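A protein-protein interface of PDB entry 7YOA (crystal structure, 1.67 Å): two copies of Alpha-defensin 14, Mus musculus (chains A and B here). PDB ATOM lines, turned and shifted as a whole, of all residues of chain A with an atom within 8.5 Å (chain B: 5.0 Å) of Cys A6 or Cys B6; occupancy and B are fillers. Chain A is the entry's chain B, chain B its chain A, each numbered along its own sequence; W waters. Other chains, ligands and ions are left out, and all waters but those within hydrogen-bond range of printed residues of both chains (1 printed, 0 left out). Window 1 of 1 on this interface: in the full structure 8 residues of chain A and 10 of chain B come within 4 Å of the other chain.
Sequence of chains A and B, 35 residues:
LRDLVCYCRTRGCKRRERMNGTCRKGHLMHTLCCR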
ATOM      1  N   ASP A   3      -1.041 -19.547   9.637  1.00  0.00           N
ATOM      2  CA  ASP A   3      -2.497 -19.393   9.577  1.00  0.00           C
ATOM      3  C   ASP A   3      -3.115 -19.159  10.962  1.00  0.00           C
ATOM      4  O   ASP A   3      -2.666 -19.714  11.969  1.00  0.00           O
ATOM      5  CB  ASP A   3      -3.137 -20.622   8.938  1.00  0.00           C
ATOM      6  CG  ASP A   3      -2.368 -21.104   7.734  1.00  0.00           C
ATOM      7  OD1 ASP A   3      -2.635 -20.590   6.626  1.00  0.00           O
ATOM      8  OD2 ASP A   3      -1.479 -21.970   7.908  1.00  0.00           O
ATOM      9  N   LEU A   4      -4.159 -18.340  10.988  1.00  0.00           N
ATOM     10  CA  LEU A   4      -4.841 -17.942  12.213  1.00  0.00           C
ATOM     11  C   LEU A   4      -6.255 -18.517  12.201  1.00  0.00           C
ATOM     12  O   LEU A   4      -6.938 -18.454  11.171  1.00  0.00           O
ATOM     13  CB  LEU A   4      -4.892 -16.419  12.300  1.00  0.00           C
ATOM     14  CG  LEU A   4      -5.063 -15.685  13.621  1.00  0.00           C
ATOM     15  CD1 LEU A   4      -3.952 -15.995  14.606  1.00  0.00           C
ATOM     16  CD2 LEU A   4      -5.123 -14.207  13.345  1.00  0.00           C
ATOM     17  N   VAL A   5      -6.701 -19.067  13.335  1.00  0.00           N
ATOM     18  CA  VAL A   5      -8.077 -19.537  13.463  1.00  0.00           C
ATOM     19  C   VAL A   5      -8.682 -18.748  14.606  1.00  0.00           C
ATOM     20  O   VAL A   5      -8.073 -18.653  15.682  1.00  0.00           O
ATOM     21  CB  VAL A   5      -8.177 -21.050  13.722  1.00  0.00           C
ATOM     22  CG1 VAL A   5      -9.664 -21.465  13.871  1.00  0.00           C
ATOM     23  CG2 VAL A   5      -7.525 -21.856  12.557  1.00  0.00           C
ATOM     24  N   CYS A   6      -9.822 -18.135  14.344  1.00  0.00           N
ATOM     25  CA  CYS A   6     -10.486 -17.246  15.284  1.00  0.00           C
ATOM     26  C   CYS A   6     -11.847 -17.783  15.673  1.00  0.00           C
ATOM     27  O   CYS A   6     -12.597 -18.253  14.817  1.00  0.00           O
ATOM     28  CB  CYS A   6     -10.673 -15.864  14.692  1.00  0.00           C
ATOM     29  SG  CYS A   6      -9.050 -15.107  14.242  1.00  0.00           S
ATOM     30  N   TYR A   7     -12.182 -17.630  16.976  1.00  0.00           N
ATOM     31  CA  TYR A   7     -13.462 -18.022  17.536  1.00  0.00           C
ATOM     32  C   TYR A   7     -14.090 -16.792  18.155  1.00  0.00           C
ATOM     33  O   TYR A   7     -13.392 -16.038  18.841  1.00  0.00           O
ATOM     34  CB  TYR A   7     -13.327 -19.088  18.612  1.00  0.00           C
ATOM     35  CG  TYR A   7     -12.591 -20.332  18.151  1.00  0.00           C
ATOM     36  CD1 TYR A   7     -11.195 -20.345  18.101  1.00  0.00           C
ATOM     37  CD2 TYR A   7     -13.272 -21.482  17.825  1.00  0.00           C
ATOM     38  CE1 TYR A   7     -10.488 -21.446  17.698  1.00  0.00           C
ATOM     39  CE2 TYR A   7     -12.544 -22.622  17.405  1.00  0.00           C
ATOM     40  CZ  TYR A   7     -11.154 -22.573  17.353  1.00  0.00           C
ATOM     41  OH  TYR A   7     -10.384 -23.682  16.954  1.00  0.00           O
ATOM     42  N   CYS A   8     -15.374 -16.605  17.915  1.00  0.00           N
ATOM     43  CA  CYS A   8     -16.132 -15.540  18.586  1.00  0.00           C
ATOM     44  C   CYS A   8     -16.682 -16.139  19.884  1.00  0.00           C
ATOM     45  O   CYS A   8     -17.619 -16.950  19.845  1.00  0.00           O
ATOM     46  CB  CYS A   8     -17.253 -15.039  17.688  1.00  0.00           C
ATOM     47  SG  CYS A   8     -18.043 -13.569  18.359  1.00  0.00           S
ATOM     48  N   ARG A   9     -16.065 -15.811  21.021  1.00  0.00           N
ATOM     49  CA  ARG A   9     -16.302 -16.557  22.249  1.00  0.00           C
ATOM     50  C   ARG A   9     -17.212 -15.793  23.202  1.00  0.00           C
ATOM     51  O   ARG A   9     -16.990 -14.606  23.460  1.00  0.00           O
ATOM     52  CB  ARG A   9     -14.991 -16.900  22.954  1.00  0.00           C
ATOM     53  CG  ARG A   9     -14.085 -17.867  22.096  1.00  0.00           C
ATOM     54  CD  ARG A   9     -13.090 -18.540  22.940  1.00  0.00           C
ATOM     55  NE  ARG A   9     -12.306 -19.536  22.219  1.00  0.00           N
ATOM     56  CZ  ARG A   9     -12.688 -20.781  21.956  1.00  0.00           C
ATOM     57  NH1 ARG A   9     -13.873 -21.245  22.330  1.00  0.00           N
ATOM     58  NH2 ARG A   9     -11.831 -21.600  21.349  1.00  0.00           N
ATOM     59  N   GLU A  17      -5.018 -18.268  23.511  1.00  0.00           N
ATOM     60  CA  GLU A  17      -5.536 -17.428  22.441  1.00  0.00           C
ATOM     61  C   GLU A  17      -5.243 -15.973  22.772  1.00  0.00           C
ATOM     62  O   GLU A  17      -4.872 -15.625  23.897  1.00  0.00           O
ATOM     63  CB  GLU A  17      -7.048 -17.631  22.273  1.00  0.00           C
ATOM     64  CG  GLU A  17      -7.433 -19.070  22.025  1.00  0.00           C
ATOM     65  CD  GLU A  17      -8.911 -19.276  21.912  1.00  0.00           C
ATOM     66  OE1 GLU A  17      -9.684 -18.633  22.682  1.00  0.00           O
ATOM     67  OE2 GLU A  17      -9.312 -20.188  21.163  1.00  0.00           O
ATOM     68  N   ARG A  18      -5.452 -15.109  21.796  1.00  0.00           N
ATOM     69  CA  ARG A  18      -5.331 -13.684  22.054  1.00  0.00           C
ATOM     70  C   ARG A  18      -6.523 -12.995  21.429  1.00  0.00           C
ATOM     71  O   ARG A  18      -6.973 -13.387  20.344  1.00  0.00           O
ATOM     72  CB  ARG A  18      -4.022 -13.121  21.490  1.00  0.00           C
ATOM     73  CG  ARG A  18      -2.807 -13.631  22.243  1.00  0.00           C
ATOM     74  CD  ARG A  18      -1.541 -12.868  21.919  1.00  0.00           C
ATOM     75  NE  ARG A  18      -1.593 -11.479  22.349  1.00  0.00           N
ATOM     76  CZ  ARG A  18      -0.867 -10.982  23.344  1.00  0.00           C
ATOM     77  NH1 ARG A  18      -0.035 -11.741  24.035  1.00  0.00           N
ATOM     78  NH2 ARG A  18      -0.981  -9.691  23.655  1.00  0.00           N
ATOM     79  N   MET A  19      -7.049 -11.992  22.126  1.00  0.00           N
ATOM     80  CA  MET A  19      -8.082 -11.181  21.535  1.00  0.00           C
ATOM     81  C   MET A  19      -7.568 -10.681  20.186  1.00  0.00           C
ATOM     82  O   MET A  19      -6.352 -10.665  19.908  1.00  0.00           O
ATOM     83  CB  MET A  19      -8.428 -10.030  22.483  1.00  0.00           C
ATOM     84  CG  MET A  19      -9.829  -9.462  22.312  1.00  0.00           C
ATOM     85  SD  MET A  19     -10.222  -8.284  23.652  1.00  0.00           S
ATOM     86  CE  MET A  19     -11.633  -7.383  22.980  1.00  0.00           C
ATOM     87  N   ASN A  20      -8.495 -10.427  19.290  1.00  0.00           N
ATOM     88  CA  ASN A  20      -8.130  -9.843  18.028  1.00  0.00           C
ATOM     89  C   ASN A  20      -9.263  -8.924  17.613  1.00  0.00           C
ATOM     90  O   ASN A  20      -9.917  -9.123  16.594  1.00  0.00           O
ATOM     91  CB  ASN A  20      -7.886 -10.940  17.008  1.00  0.00           C
ATOM     92  CG  ASN A  20      -6.863 -10.559  15.959  1.00  0.00           C
ATOM     93  OD1 ASN A  20      -6.984  -9.540  15.278  1.00  0.00           O
ATOM     94  ND2 ASN A  20      -5.864 -11.389  15.810  1.00  0.00           N
ATOM     95  N   GLY A  21      -9.558  -7.964  18.441  1.00  0.00           N
ATOM     96  CA  GLY A  21     -10.802  -7.225  18.290  1.00  0.00           C
ATOM     97  C   GLY A  21     -12.045  -7.922  18.834  1.00  0.00           C
ATOM     98  O   GLY A  21     -12.011  -8.860  19.662  1.00  0.00           O
ATOM     99  N   CYS A  23     -16.303  -9.236  17.975  1.00  0.00           N
ATOM    100  CA  CYS A  23     -17.143  -9.903  16.997  1.00  0.00           C
ATOM    101  C   CYS A  23     -18.571  -9.868  17.519  1.00  0.00           C
ATOM    102  O   CYS A  23     -18.803  -9.621  18.696  1.00  0.00           O
ATOM    103  CB  CYS A  23     -16.683 -11.337  16.782  1.00  0.00           C
ATOM    104  SG  CYS A  23     -16.512 -12.245  18.301  1.00  0.00           S
ATOM    105  N   THR A  31     -15.675 -11.055  22.504  1.00  0.00           N
ATOM    106  CA  THR A  31     -14.276 -11.104  22.113  1.00  0.00           C
ATOM    107  C   THR A  31     -14.102 -12.032  20.906  1.00  0.00           C
ATOM    108  O   THR A  31     -14.553 -13.185  20.952  1.00  0.00           O
ATOM    109  CB  THR A  31     -13.441 -11.697  23.225  1.00  0.00           C
ATOM    110  OG1 THR A  31     -14.075 -12.913  23.639  1.00  0.00           O
ATOM    111  CG2 THR A  31     -13.425 -10.753  24.414  1.00  0.00           C
ATOM    112  N   LEU A  32     -13.316 -11.591  19.928  1.00  0.00           N
ATOM    113  CA  LEU A  32     -12.798 -12.504  18.894  1.00  0.00           C
ATOM    114  C   LEU A  32     -11.439 -13.017  19.385  1.00  0.00           C
ATOM    115  O   LEU A  32     -10.550 -12.228  19.704  1.00  0.00           O
ATOM    116  CB  LEU A  32     -12.645 -11.814  17.532  1.00  0.00           C
ATOM    117  CG  LEU A  32     -12.209 -12.706  16.357  1.00  0.00           C
ATOM    118  CD1 LEU A  32     -13.380 -13.608  15.935  1.00  0.00           C
ATOM    119  CD2 LEU A  32     -11.711 -11.831  15.248  1.00  0.00           C
ATOM    120  N   CYS A  33     -11.250 -14.330  19.403  1.00  0.00           N
ATOM    121  CA  CYS A  33     -10.107 -14.952  20.046  1.00  0.00           C
ATOM    122  C   CYS A  33      -9.412 -15.828  19.046  1.00  0.00           C
ATOM    123  O   CYS A  33     -10.053 -16.717  18.516  1.00  0.00           O
ATOM    124  CB  CYS A  33     -10.568 -15.817  21.212  1.00  0.00           C
ATOM    125  SG  CYS A  33     -11.546 -14.835  22.371  1.00  0.00           S
ATOM    126  N   CYS A  34      -8.126 -15.589  18.799  1.00  0.00           N
ATOM    127  CA  CYS A  34      -7.432 -16.270  17.716  1.00  0.00           C
ATOM    128  C   CYS A  34      -6.168 -16.939  18.231  1.00  0.00           C
ATOM    129  O   CYS A  34      -5.553 -16.479  19.203  1.00  0.00           O
ATOM    130  CB  CYS A  34      -7.068 -15.290  16.582  1.00  0.00           C
ATOM    131  SG  CYS A  34      -8.395 -14.256  16.010  1.00  0.00           S
ATOM    132  N   ARG A  35      -5.782 -17.999  17.533  1.00  0.00           N
ATOM    133  CA  ARG A  35      -4.534 -18.734  17.775  1.00  0.00           C
ATOM    134  C   ARG A  35      -4.020 -19.332  16.464  1.00  0.00           C
ATOM    135  O   ARG A  35      -4.782 -19.561  15.523  1.00  0.00           O
ATOM    136  CB  ARG A  35      -4.730 -19.821  18.836  1.00  0.00           C
ATOM    137  CG  ARG A  35      -3.430 -20.403  19.341  1.00  0.00           C
ATOM    138  CD  ARG A  35      -3.662 -21.795  19.901  1.00  0.00           C
ATOM    139  NE  ARG A  35      -2.680 -22.183  20.905  1.00  0.00           N
ATOM    140  CZ  ARG A  35      -1.796 -23.150  20.680  1.00  0.00           C
ATOM    141  NH1 ARG A  35      -1.794 -23.828  19.539  1.00  0.00           N
ATOM    142  NH2 ARG A  35      -0.882 -23.434  21.608  1.00  0.00           N
ATOM    143  OXT ARG A  35      -2.826 -19.605  16.306  1.00  0.00           O
ATOM    144  N   LEU B   4      -3.569 -17.050   5.977  1.00  0.00           N
ATOM    145  CA  LEU B   4      -5.008 -17.127   5.836  1.00  0.00           C
ATOM    146  C   LEU B   4      -5.572 -16.740   7.189  1.00  0.00           C
ATOM    147  O   LEU B   4      -5.022 -17.166   8.204  1.00  0.00           O
ATOM    148  CB  LEU B   4      -5.425 -18.553   5.483  1.00  0.00           C
ATOM    149  CG  LEU B   4      -6.040 -18.787   4.114  1.00  0.00           C
ATOM    150  CD1 LEU B   4      -6.504 -20.211   4.051  1.00  0.00           C
ATOM    151  CD2 LEU B   4      -7.154 -17.786   3.809  1.00  0.00           C
ATOM    152  N   VAL B   5      -6.643 -15.950   7.220  1.00  0.00           N
ATOM    153  CA  VAL B   5      -7.368 -15.721   8.477  1.00  0.00           C
ATOM    154  C   VAL B   5      -8.675 -16.500   8.406  1.00  0.00           C
ATOM    155  O   VAL B   5      -9.480 -16.293   7.486  1.00  0.00           O
ATOM    156  CB  VAL B   5      -7.652 -14.242   8.730  1.00  0.00           C
ATOM    157  CG1 VAL B   5      -8.536 -14.104   9.983  1.00  0.00           C
ATOM    158  CG2 VAL B   5      -6.350 -13.473   8.836  1.00  0.00           C
ATOM    159  N   CYS B   6      -8.913 -17.361   9.393  1.00  0.00           N
ATOM    160  CA  CYS B   6     -10.078 -18.235   9.384  1.00  0.00           C
ATOM    161  C   CYS B   6     -10.914 -18.003  10.637  1.00  0.00           C
ATOM    162  O   CYS B   6     -10.371 -17.791  11.720  1.00  0.00           O
ATOM    163  CB  CYS B   6      -9.667 -19.694   9.315  1.00  0.00           C
ATOM    164  SG  CYS B   6      -8.648 -20.070   7.852  1.00  0.00           S
ATOM    165  N   TYR B   7     -12.230 -18.059  10.466  1.00  0.00           N
ATOM    166  CA  TYR B   7     -13.221 -17.944  11.526  1.00  0.00           C
ATOM    167  C   TYR B   7     -13.911 -19.285  11.673  1.00  0.00           C
ATOM    168  O   TYR B   7     -14.271 -19.923  10.667  1.00  0.00           O
ATOM    169  CB  TYR B   7     -14.227 -16.849  11.186  1.00  0.00           C
ATOM    170  CG  TYR B   7     -13.527 -15.546  10.932  1.00  0.00           C
ATOM    171  CD1 TYR B   7     -13.277 -14.685  11.966  1.00  0.00           C
ATOM    172  CD2 TYR B   7     -13.065 -15.203   9.649  1.00  0.00           C
ATOM    173  CE1 TYR B   7     -12.616 -13.472  11.750  1.00  0.00           C
ATOM    174  CE2 TYR B   7     -12.390 -14.004   9.421  1.00  0.00           C
ATOM    175  CZ  TYR B   7     -12.168 -13.152  10.471  1.00  0.00           C
ATOM    176  OH  TYR B   7     -11.502 -11.958  10.252  1.00  0.00           O
ATOM    177  N   CYS B   8     -14.041 -19.760  12.897  1.00  0.00           N
ATOM    178  CA  CYS B   8     -14.745 -21.022  13.149  1.00  0.00           C
ATOM    179  C   CYS B   8     -16.183 -20.680  13.505  1.00  0.00           C
ATOM    180  O   CYS B   8     -16.453 -20.189  14.609  1.00  0.00           O
ATOM    181  CB  CYS B   8     -14.073 -21.807  14.266  1.00  0.00           C
ATOM    182  SG  CYS B   8     -14.724 -23.473  14.528  1.00  0.00           S
ATOM    183  N   ASN B  20     -13.369 -23.799   4.262  1.00  0.00           N
ATOM    184  CA  ASN B  20     -12.095 -24.508   4.269  1.00  0.00           C
ATOM    185  C   ASN B  20     -12.184 -25.714   5.188  1.00  0.00           C
ATOM    186  O   ASN B  20     -11.295 -25.916   6.030  1.00  0.00           O
ATOM    187  CB  ASN B  20     -10.951 -23.586   4.671  1.00  0.00           C
ATOM    188  CG  ASN B  20      -9.574 -24.128   4.270  1.00  0.00           C
ATOM    189  OD1 ASN B  20      -9.452 -25.016   3.405  1.00  0.00           O
ATOM    190  ND2 ASN B  20      -8.532 -23.586   4.884  1.00  0.00           N
ATOM    191  N   LEU B  32     -15.163 -23.897   9.054  1.00  0.00           N
ATOM    192  CA  LEU B  32     -13.938 -23.106   8.998  1.00  0.00           C
ATOM    193  C   LEU B  32     -14.026 -22.196   7.772  1.00  0.00           C
ATOM    194  O   LEU B  32     -13.989 -22.686   6.643  1.00  0.00           O
ATOM    195  CB  LEU B  32     -12.698 -24.007   8.956  1.00  0.00           C
ATOM    196  CG  LEU B  32     -11.427 -23.190   9.220  1.00  0.00           C
ATOM    197  CD1 LEU B  32     -11.441 -22.632  10.641  1.00  0.00           C
ATOM    198  CD2 LEU B  32     -10.106 -23.961   8.958  1.00  0.00           C
ATOM    199  N   CYS B  33     -14.163 -20.884   7.996  1.00  0.00           N
ATOM    200  CA  CYS B  33     -14.391 -19.914   6.918  1.00  0.00           C
ATOM    201  C   CYS B  33     -13.196 -18.995   6.818  1.00  0.00           C
ATOM    202  O   CYS B  33     -12.887 -18.265   7.767  1.00  0.00           O
ATOM    203  CB  CYS B  33     -15.658 -19.103   7.153  1.00  0.00           C
ATOM    204  SG  CYS B  33     -17.082 -20.128   7.374  1.00  0.00           S
ATOM    205  N   CYS B  34     -12.542 -18.995   5.671  1.00  0.00           N
ATOM    206  CA  CYS B  34     -11.267 -18.318   5.583  1.00  0.00           C
ATOM    207  C   CYS B  34     -11.300 -17.225   4.523  1.00  0.00           C
ATOM    208  O   CYS B  34     -12.046 -17.293   3.539  1.00  0.00           O
ATOM    209  CB  CYS B  34     -10.135 -19.304   5.275  1.00  0.00           C
ATOM    210  SG  CYS B  34      -9.961 -20.679   6.454  1.00  0.00           S
HETATM  211  O   HOH W   1     -16.930 -18.686  16.505  1.00  0.00           O
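Among the printed residues, pairs that only touch across the chains: Cys A6 with Tyr B7 (3.4 Å), Val A5 with Cys B6 (3.4 Å), Tyr A7 with Cys B8 (3.6 Å), Asp A3 with Leu B4 (3.6 Å), Leu A4 with Val B5 (3.8 Å), Val A5 with Leu B32 (3.9 Å) and Leu A32 with Tyr B7 (3.97 Å).
O of Leu B4 sits at hydrogen-bond distance from N of Leu A4 (3.1 Å). N of Cys B6 is in hydrogen-bond range of O of Leu A4, at 2.9 Å. The backbone NH (N) of Cys A6 sits at hydrogen-bond distance from the backbone carbonyl oxygen (O) of Cys B6, 2.7 Å away. The backbone NH (N) of Cys B8 is in hydrogen-bond range of the backbone carbonyl oxygen (O) of Cys A6, at 2.8 Å.
Of the 18 printed residues of chain A, 6 touch a printed residue of chain B. Hydrophobic or aromatic side chains of chain A within 4 Å of the printed part of chain B: Val A5, Tyr A7 and Leu A32. Along chain A the printed residues that touch a printed residue of chain B span positions 3 to 32. Hydrophobic or aromatic side chains of chain B within 4 Å of the printed part of chain A: Leu B4, Tyr B7 and Leu B32. Along chain B the printed residues that touch a printed residue of chain A span positions 4 to 32.
Water W1 lies within hydrogen-bond range of the backbone carbonyl oxygen (O) of Cys B8 and the backbone NH (N) of Cys A8.
Cys A6 touches just these residues of chain B: Cys B6 (2.7 Å), Tyr B7 (3.4 Å) and Cys B8 (2.8 Å). Cys B6 touches just these residues of chain A: Leu A4, Val A5 and Cys A6. Printed residues of chain A within 4 Å of Cys B8: Cys A6 and Tyr A7. Printed residues of chain A within 4 Å of Leu B32: Val A5. The nearest residue of chain B that does not touch Cys A6 is Val B5 (4.4 Å).
The side-chain sulfur of Cys B34 forms a disulfide with the side-chain sulfur of Cys B6, at 2.0 Å. The backbone NH (N) of Val A5 lies within hydrogen-bond range of the chain-end carboxylate (O) of Arg A35, at 3.0 Å. The backbone carbonyl oxygen of Cys A33 lies within hydrogen-bond range of the backbone NH of Tyr A7, at 2.8 Å. The backbone NH of Asn A20 lies within hydrogen-bond range of the backbone carbonyl oxygen of Leu A32, 2.8 Å away. SG of Cys A23 sits at hydrogen-bond distance from N of Leu A32 (3.6 Å). The side-chain sulfur of Cys A8 forms a disulfide with the side-chain sulfur of Cys A23 (2.0 Å).
Leu A4 touches Cys B6, but with the chains exchanged Cys A6 does not touch Leu B4 (7.5 Å). Val A5 touches Leu B32, but with the chains exchanged Leu A32 does not touch Val B5 (6.6 Å). Cys A6 touches Cys B8, but with the chains exchanged Cys A8 does not touch Cys B6 (8.1 Å). Tyr A7 touches Cys B8, but with the chains exchanged Cys A8 does not touch Tyr B7 (6.6 Å). Of the 11 pairs that touch across the chains among the printed residues, 2 have their exchanged pair printed and touching as well.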
